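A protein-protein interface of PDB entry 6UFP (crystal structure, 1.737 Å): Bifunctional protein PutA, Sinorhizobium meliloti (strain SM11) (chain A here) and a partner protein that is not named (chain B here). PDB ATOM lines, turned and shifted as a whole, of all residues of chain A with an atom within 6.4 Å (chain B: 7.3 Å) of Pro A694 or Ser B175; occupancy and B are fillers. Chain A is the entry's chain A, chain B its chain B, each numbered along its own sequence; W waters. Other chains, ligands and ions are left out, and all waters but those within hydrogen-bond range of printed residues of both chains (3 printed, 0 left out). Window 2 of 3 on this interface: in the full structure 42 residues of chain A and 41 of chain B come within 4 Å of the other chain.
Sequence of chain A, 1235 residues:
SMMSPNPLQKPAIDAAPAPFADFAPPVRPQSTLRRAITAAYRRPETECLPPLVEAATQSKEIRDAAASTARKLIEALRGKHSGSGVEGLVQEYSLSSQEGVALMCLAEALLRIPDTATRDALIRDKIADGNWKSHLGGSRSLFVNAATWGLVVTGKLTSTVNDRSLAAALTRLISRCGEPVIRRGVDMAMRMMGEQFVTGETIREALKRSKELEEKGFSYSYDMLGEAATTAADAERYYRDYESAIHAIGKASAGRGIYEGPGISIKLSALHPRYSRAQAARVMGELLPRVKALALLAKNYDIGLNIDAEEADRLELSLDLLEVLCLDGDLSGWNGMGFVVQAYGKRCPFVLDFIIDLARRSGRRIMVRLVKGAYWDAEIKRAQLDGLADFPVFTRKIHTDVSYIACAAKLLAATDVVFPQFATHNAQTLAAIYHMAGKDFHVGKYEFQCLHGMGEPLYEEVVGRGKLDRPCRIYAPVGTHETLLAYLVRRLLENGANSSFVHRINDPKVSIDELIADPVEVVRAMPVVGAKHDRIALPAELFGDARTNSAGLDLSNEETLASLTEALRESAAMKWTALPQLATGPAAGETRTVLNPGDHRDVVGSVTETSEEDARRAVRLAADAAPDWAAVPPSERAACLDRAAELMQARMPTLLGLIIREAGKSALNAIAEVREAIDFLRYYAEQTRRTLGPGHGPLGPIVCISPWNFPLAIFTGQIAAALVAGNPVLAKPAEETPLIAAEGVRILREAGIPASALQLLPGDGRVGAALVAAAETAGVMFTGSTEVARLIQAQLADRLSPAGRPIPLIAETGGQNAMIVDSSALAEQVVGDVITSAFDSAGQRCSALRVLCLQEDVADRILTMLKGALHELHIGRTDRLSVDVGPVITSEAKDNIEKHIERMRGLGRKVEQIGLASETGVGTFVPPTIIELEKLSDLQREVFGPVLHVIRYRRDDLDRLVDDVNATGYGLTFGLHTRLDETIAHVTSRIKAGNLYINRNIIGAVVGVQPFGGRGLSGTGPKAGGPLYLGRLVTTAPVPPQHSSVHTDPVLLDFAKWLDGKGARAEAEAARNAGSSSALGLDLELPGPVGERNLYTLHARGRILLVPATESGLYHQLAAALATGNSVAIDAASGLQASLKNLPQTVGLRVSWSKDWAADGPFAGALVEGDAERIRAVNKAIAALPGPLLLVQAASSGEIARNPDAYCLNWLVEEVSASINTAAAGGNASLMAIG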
ATOM      1  N   PRO A 634      26.751   5.595  13.313  1.00  0.00           N
ATOM      2  CA  PRO A 634      25.324   5.487  12.966  1.00  0.00           C
ATOM      3  C   PRO A 634      24.417   5.298  14.171  1.00  0.00           C
ATOM      4  O   PRO A 634      23.299   5.822  14.179  1.00  0.00           O
ATOM      5  CB  PRO A 634      25.291   4.275  12.025  1.00  0.00           C
ATOM      6  CG  PRO A 634      26.657   4.239  11.416  1.00  0.00           C
ATOM      7  CD  PRO A 634      27.603   4.732  12.473  1.00  0.00           C
ATOM      8  N   THR A 691      21.180  -1.655   9.910  1.00  0.00           N
ATOM      9  CA  THR A 691      21.865  -1.809   8.619  1.00  0.00           C
ATOM     10  C   THR A 691      23.211  -1.102   8.475  1.00  0.00           C
ATOM     11  O   THR A 691      24.116  -1.665   7.859  1.00  0.00           O
ATOM     12  CB  THR A 691      20.965  -1.311   7.471  1.00  0.00           C
ATOM     13  OG1 THR A 691      20.650   0.076   7.676  1.00  0.00           O
ATOM     14  CG2 THR A 691      19.680  -2.127   7.371  1.00  0.00           C
ATOM     15  N   LEU A 692      23.354   0.136   8.947  1.00  0.00           N
ATOM     16  CA  LEU A 692      24.441   0.984   8.454  1.00  0.00           C
ATOM     17  C   LEU A 692      25.770   0.686   9.149  1.00  0.00           C
ATOM     18  O   LEU A 692      25.845   0.602  10.382  1.00  0.00           O
ATOM     19  CB  LEU A 692      24.081   2.465   8.614  1.00  0.00           C
ATOM     20  CG  LEU A 692      22.954   2.973   7.706  1.00  0.00           C
ATOM     21  CD1 LEU A 692      22.885   4.495   7.726  1.00  0.00           C
ATOM     22  CD2 LEU A 692      23.133   2.480   6.279  1.00  0.00           C
ATOM     23  N   GLY A 693      26.817   0.532   8.349  1.00  0.00           N
ATOM     24  CA  GLY A 693      28.144   0.297   8.865  1.00  0.00           C
ATOM     25  C   GLY A 693      29.157   1.206   8.200  1.00  0.00           C
ATOM     26  O   GLY A 693      28.800   2.136   7.470  1.00  0.00           O
ATOM     27  N   PRO A 694      30.447   0.938   8.431  1.00  0.00           N
ATOM     28  CA  PRO A 694      31.496   1.837   7.914  1.00  0.00           C
ATOM     29  C   PRO A 694      31.582   1.897   6.398  1.00  0.00           C
ATOM     30  O   PRO A 694      31.973   2.935   5.852  1.00  0.00           O
ATOM     31  CB  PRO A 694      32.779   1.256   8.523  1.00  0.00           C
ATOM     32  CG  PRO A 694      32.322   0.499   9.727  1.00  0.00           C
ATOM     33  CD  PRO A 694      30.988  -0.071   9.358  1.00  0.00           C
ATOM     34  N   GLY A 695      31.233   0.821   5.693  1.00  0.00           N
ATOM     35  CA  GLY A 695      31.322   0.821   4.244  1.00  0.00           C
ATOM     36  C   GLY A 695      30.175   1.489   3.514  1.00  0.00           C
ATOM     37  O   GLY A 695      30.243   1.642   2.293  1.00  0.00           O
ATOM     38  N   HIS A 696      29.114   1.887   4.217  1.00  0.00           N
ATOM     39  CA  HIS A 696      27.998   2.581   3.578  1.00  0.00           C
ATOM     40  C   HIS A 696      28.202   4.076   3.809  1.00  0.00           C
ATOM     41  O   HIS A 696      27.674   4.666   4.753  1.00  0.00           O
ATOM     42  CB  HIS A 696      26.667   2.090   4.131  1.00  0.00           C
ATOM     43  CG  HIS A 696      26.590   0.602   4.264  1.00  0.00           C
ATOM     44  ND1 HIS A 696      26.525  -0.033   5.486  1.00  0.00           N
ATOM     45  CD2 HIS A 696      26.590  -0.378   3.327  1.00  0.00           C
ATOM     46  CE1 HIS A 696      26.482  -1.340   5.296  1.00  0.00           C
ATOM     47  NE2 HIS A 696      26.511  -1.575   3.996  1.00  0.00           N
ATOM     48  N   GLY A 697      29.004   4.683   2.940  1.00  0.00           N
ATOM     49  CA  GLY A 697      29.374   6.068   3.093  1.00  0.00           C
ATOM     50  C   GLY A 697      28.288   7.017   2.631  1.00  0.00           C
ATOM     51  O   GLY A 697      27.556   6.750   1.673  1.00  0.00           O
ATOM     52  N   PRO A1038      23.170  -0.827   1.879  1.00  0.00           N
ATOM     53  CA  PRO A1038      23.222  -2.019   2.728  1.00  0.00           C
ATOM     54  C   PRO A1038      22.123  -3.008   2.347  1.00  0.00           C
ATOM     55  O   PRO A1038      21.241  -2.724   1.539  1.00  0.00           O
ATOM     56  CB  PRO A1038      22.993  -1.453   4.129  1.00  0.00           C
ATOM     57  CG  PRO A1038      22.059  -0.291   3.880  1.00  0.00           C
ATOM     58  CD  PRO A1038      22.480   0.297   2.544  1.00  0.00           C
ATOM     59  N   ILE B 127      37.115 -12.380   5.772  1.00  0.00           N
ATOM     60  CA  ILE B 127      35.718 -12.442   6.188  1.00  0.00           C
ATOM     61  C   ILE B 127      35.243 -11.079   6.675  1.00  0.00           C
ATOM     62  O   ILE B 127      34.162 -10.612   6.300  1.00  0.00           O
ATOM     63  CB  ILE B 127      35.522 -13.513   7.274  1.00  0.00           C
ATOM     64  CG1 ILE B 127      36.248 -14.815   6.906  1.00  0.00           C
ATOM     65  CG2 ILE B 127      34.035 -13.754   7.502  1.00  0.00           C
ATOM     66  CD1 ILE B 127      35.716 -15.485   5.674  1.00  0.00           C
ATOM     67  N   ALA B 128      36.034 -10.426   7.529  1.00  0.00           N
ATOM     68  CA  ALA B 128      35.590  -9.170   8.124  1.00  0.00           C
ATOM     69  C   ALA B 128      35.386  -8.075   7.086  1.00  0.00           C
ATOM     70  O   ALA B 128      34.746  -7.061   7.386  1.00  0.00           O
ATOM     71  CB  ALA B 128      36.583  -8.708   9.189  1.00  0.00           C
ATOM     72  N   ASP B 129      35.905  -8.256   5.872  1.00  0.00           N
ATOM     73  CA  ASP B 129      35.687  -7.324   4.774  1.00  0.00           C
ATOM     74  C   ASP B 129      34.576  -7.791   3.841  1.00  0.00           C
ATOM     75  O   ASP B 129      34.631  -7.540   2.633  1.00  0.00           O
ATOM     76  CB  ASP B 129      36.986  -7.104   3.997  1.00  0.00           C
ATOM     77  CG  ASP B 129      38.070  -6.461   4.843  1.00  0.00           C
ATOM     78  OD1 ASP B 129      37.746  -5.594   5.684  1.00  0.00           O
ATOM     79  OD2 ASP B 129      39.251  -6.826   4.668  1.00  0.00           O
ATOM     80  N   GLY B 130      33.575  -8.487   4.378  1.00  0.00           N
ATOM     81  CA  GLY B 130      32.408  -8.868   3.609  1.00  0.00           C
ATOM     82  C   GLY B 130      32.616 -10.010   2.635  1.00  0.00           C
ATOM     83  O   GLY B 130      31.665 -10.725   2.303  1.00  0.00           O
ATOM     84  N   ALA B 169      21.354 -12.014   5.820  1.00  0.00           N
ATOM     85  CA  ALA B 169      21.578 -11.665   7.222  1.00  0.00           C
ATOM     86  C   ALA B 169      23.072 -11.645   7.551  1.00  0.00           C
ATOM     87  O   ALA B 169      23.542 -10.791   8.307  1.00  0.00           O
ATOM     88  CB  ALA B 169      20.837 -12.644   8.132  1.00  0.00           C
ATOM     89  N   LEU B 170      23.831 -12.569   6.974  1.00  0.00           N
ATOM     90  CA  LEU B 170      25.257 -12.619   7.275  1.00  0.00           C
ATOM     91  C   LEU B 170      25.979 -11.420   6.680  1.00  0.00           C
ATOM     92  O   LEU B 170      26.811 -10.798   7.342  1.00  0.00           O
ATOM     93  CB  LEU B 170      25.845 -13.934   6.760  1.00  0.00           C
ATOM     94  CG  LEU B 170      27.323 -14.173   7.083  1.00  0.00           C
ATOM     95  CD1 LEU B 170      27.580 -14.049   8.563  1.00  0.00           C
ATOM     96  CD2 LEU B 170      27.654 -15.547   6.627  1.00  0.00           C
ATOM     97  N   THR B 171      25.660 -11.070   5.433  1.00  0.00           N
ATOM     98  CA  THR B 171      26.227  -9.867   4.835  1.00  0.00           C
ATOM     99  C   THR B 171      25.915  -8.632   5.679  1.00  0.00           C
ATOM    100  O   THR B 171      26.789  -7.808   5.951  1.00  0.00           O
ATOM    101  CB  THR B 171      25.690  -9.698   3.412  1.00  0.00           C
ATOM    102  OG1 THR B 171      26.037 -10.848   2.627  1.00  0.00           O
ATOM    103  CG2 THR B 171      26.248  -8.440   2.769  1.00  0.00           C
ATOM    104  N   ARG B 172      24.650  -8.487   6.085  1.00  0.00           N
ATOM    105  CA  ARG B 172      24.228  -7.324   6.854  1.00  0.00           C
ATOM    106  C   ARG B 172      24.987  -7.236   8.169  1.00  0.00           C
ATOM    107  O   ARG B 172      25.487  -6.169   8.546  1.00  0.00           O
ATOM    108  CB  ARG B 172      22.714  -7.404   7.109  1.00  0.00           C
ATOM    109  CG  ARG B 172      22.120  -6.128   7.678  1.00  0.00           C
ATOM    110  CD  ARG B 172      20.646  -6.321   8.077  1.00  0.00           C
ATOM    111  NE  ARG B 172      19.847  -7.006   7.057  1.00  0.00           N
ATOM    112  CZ  ARG B 172      19.374  -8.246   7.171  1.00  0.00           C
ATOM    113  NH1 ARG B 172      18.646  -8.786   6.201  1.00  0.00           N
ATOM    114  NH2 ARG B 172      19.631  -8.954   8.260  1.00  0.00           N
ATOM    115  N   LEU B 173      25.107  -8.365   8.865  1.00  0.00           N
ATOM    116  CA  LEU B 173      25.738  -8.381  10.177  1.00  0.00           C
ATOM    117  C   LEU B 173      27.227  -8.037  10.095  1.00  0.00           C
ATOM    118  O   LEU B 173      27.742  -7.265  10.912  1.00  0.00           O
ATOM    119  CB  LEU B 173      25.520  -9.756  10.801  1.00  0.00           C
ATOM    120  CG  LEU B 173      26.244 -10.035  12.102  1.00  0.00           C
ATOM    121  CD1 LEU B 173      25.981  -8.894  13.058  1.00  0.00           C
ATOM    122  CD2 LEU B 173      25.777 -11.361  12.671  1.00  0.00           C
ATOM    123  N   ILE B 174      27.934  -8.603   9.119  1.00  0.00           N
ATOM    124  CA  ILE B 174      29.360  -8.312   8.987  1.00  0.00           C
ATOM    125  C   ILE B 174      29.571  -6.872   8.545  1.00  0.00           C
ATOM    126  O   ILE B 174      30.464  -6.176   9.044  1.00  0.00           O
ATOM    127  CB  ILE B 174      30.029  -9.298   8.012  1.00  0.00           C
ATOM    128  CG1 ILE B 174      29.931 -10.733   8.532  1.00  0.00           C
ATOM    129  CG2 ILE B 174      31.502  -8.886   7.774  1.00  0.00           C
ATOM    130  CD1 ILE B 174      30.267 -11.768   7.494  1.00  0.00           C
ATOM    131  N   SER B 175      28.763  -6.399   7.592  1.00  0.00           N
ATOM    132  CA  SER B 175      28.920  -5.022   7.137  1.00  0.00           C
ATOM    133  C   SER B 175      28.613  -4.019   8.238  1.00  0.00           C
ATOM    134  O   SER B 175      29.142  -2.903   8.213  1.00  0.00           O
ATOM    135  CB  SER B 175      28.029  -4.734   5.922  1.00  0.00           C
ATOM    136  OG  SER B 175      28.445  -5.457   4.778  1.00  0.00           O
ATOM    137  N   ARG B 176      27.792  -4.402   9.213  1.00  0.00           N
ATOM    138  CA  ARG B 176      27.450  -3.533  10.332  1.00  0.00           C
ATOM    139  C   ARG B 176      28.475  -3.606  11.465  1.00  0.00           C
ATOM    140  O   ARG B 176      28.900  -2.568  11.979  1.00  0.00           O
ATOM    141  CB  ARG B 176      26.049  -3.899  10.844  1.00  0.00           C
ATOM    142  CG  ARG B 176      25.459  -2.969  11.891  1.00  0.00           C
ATOM    143  CD  ARG B 176      24.003  -3.354  12.188  1.00  0.00           C
ATOM    144  NE  ARG B 176      23.861  -4.568  13.005  1.00  0.00           N
ATOM    145  CZ  ARG B 176      23.260  -5.710  12.653  1.00  0.00           C
ATOM    146  NH1 ARG B 176      22.682  -5.889  11.456  1.00  0.00           N
ATOM    147  NH2 ARG B 176      23.229  -6.701  13.537  1.00  0.00           N
ATOM    148  N   CYS B 177      28.910  -4.809  11.849  1.00  0.00           N
ATOM    149  CA  CYS B 177      29.706  -4.990  13.057  1.00  0.00           C
ATOM    150  C   CYS B 177      31.120  -5.510  12.830  1.00  0.00           C
ATOM    151  O   CYS B 177      31.936  -5.407  13.745  1.00  0.00           O
ATOM    152  CB  CYS B 177      28.985  -5.938  14.027  1.00  0.00           C
ATOM    153  SG  CYS B 177      27.335  -5.362  14.505  1.00  0.00           S
ATOM    154  N   GLY B 178      31.426  -6.095  11.670  1.00  0.00           N
ATOM    155  CA  GLY B 178      32.823  -6.347  11.342  1.00  0.00           C
ATOM    156  C   GLY B 178      33.460  -7.481  12.134  1.00  0.00           C
ATOM    157  O   GLY B 178      32.796  -8.414  12.595  1.00  0.00           O
ATOM    158  N   VAL B 181      32.174  -8.967  15.895  1.00  0.00           N
ATOM    159  CA  VAL B 181      31.061  -9.891  16.048  1.00  0.00           C
ATOM    160  C   VAL B 181      31.442 -11.282  15.545  1.00  0.00           C
ATOM    161  O   VAL B 181      30.968 -12.288  16.085  1.00  0.00           O
ATOM    162  CB  VAL B 181      29.800  -9.357  15.342  1.00  0.00           C
ATOM    163  CG1 VAL B 181      29.972  -9.374  13.820  1.00  0.00           C
ATOM    164  CG2 VAL B 181      28.583 -10.176  15.755  1.00  0.00           C
HETATM  165  O   HOH W   1      26.832  -4.444   2.617  1.00  0.00           O
HETATM  166  O   HOH W   2      25.110  -3.787   6.937  1.00  0.00           O
HETATM  167  O   HOH W   3      30.451  -1.728   6.243  1.00  0.00           O
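ND1 of His A696 sits at hydrogen-bond distance from N of Gly A693 (2.9 Å). The backbone carbonyl oxygen (O) of Thr B171 sits at hydrogen-bond distance from the side-chain hydroxyl (OG) of Ser B175, at 3.1 Å.
O of Leu A692 touches CG of Arg B176, 3.9 Å away. Ser B175 touches Gly A693 (O to CA, 3.4 Å). Pro A694 touches Ser B175 (CD to O, 3.6 Å). CE1 of His A696 touches CB of Ser B175, 3.8 Å away.
Printed residues of chain B within 4 Å of Gly A693: Ser B175. Of the printed residues of chain B, His A696 touches Ser B175 (3.8 Å). Arg B172 touches none of the printed residues of chain A. Ile B174 touches none of the printed residues of chain A. Of chain A, only Gly A693 (3.4 Å), Pro A694 (3.6 Å) and His A696 (3.8 Å) come within 4 Å of Ser B175. The nearest residue of chain B that does not touch Pro A694 is Arg B176 (4.2 Å). The nearest residue of chain A that does not touch Ser B175 is Gly A695 (5.0 Å). The nearest printed residue of chain B that does not touch Leu A692 is Ser B175 (5.0 Å).
Of the 9 printed residues of chain A, 4 touch a printed residue of chain B. Printed residues of chain A that touch a printed residue of chain B: Leu A692, Gly A693, Pro A694 and His A696. Hydrophobic or aromatic side chains of chain A within 4 Å of the printed part of chain B: Pro A694 and His A696.
Water W2 bridges the backbone carbonyl oxygen of Thr A691 and the backbone carbonyl oxygen of Arg B172. Water W3 bridges the backbone carbonyl oxygen of Ser B175 and the backbone NH of Gly A695. Water W1 bridges OG of Ser B175 (2.9 Å) and NE2 of His A696 (3.2 Å).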
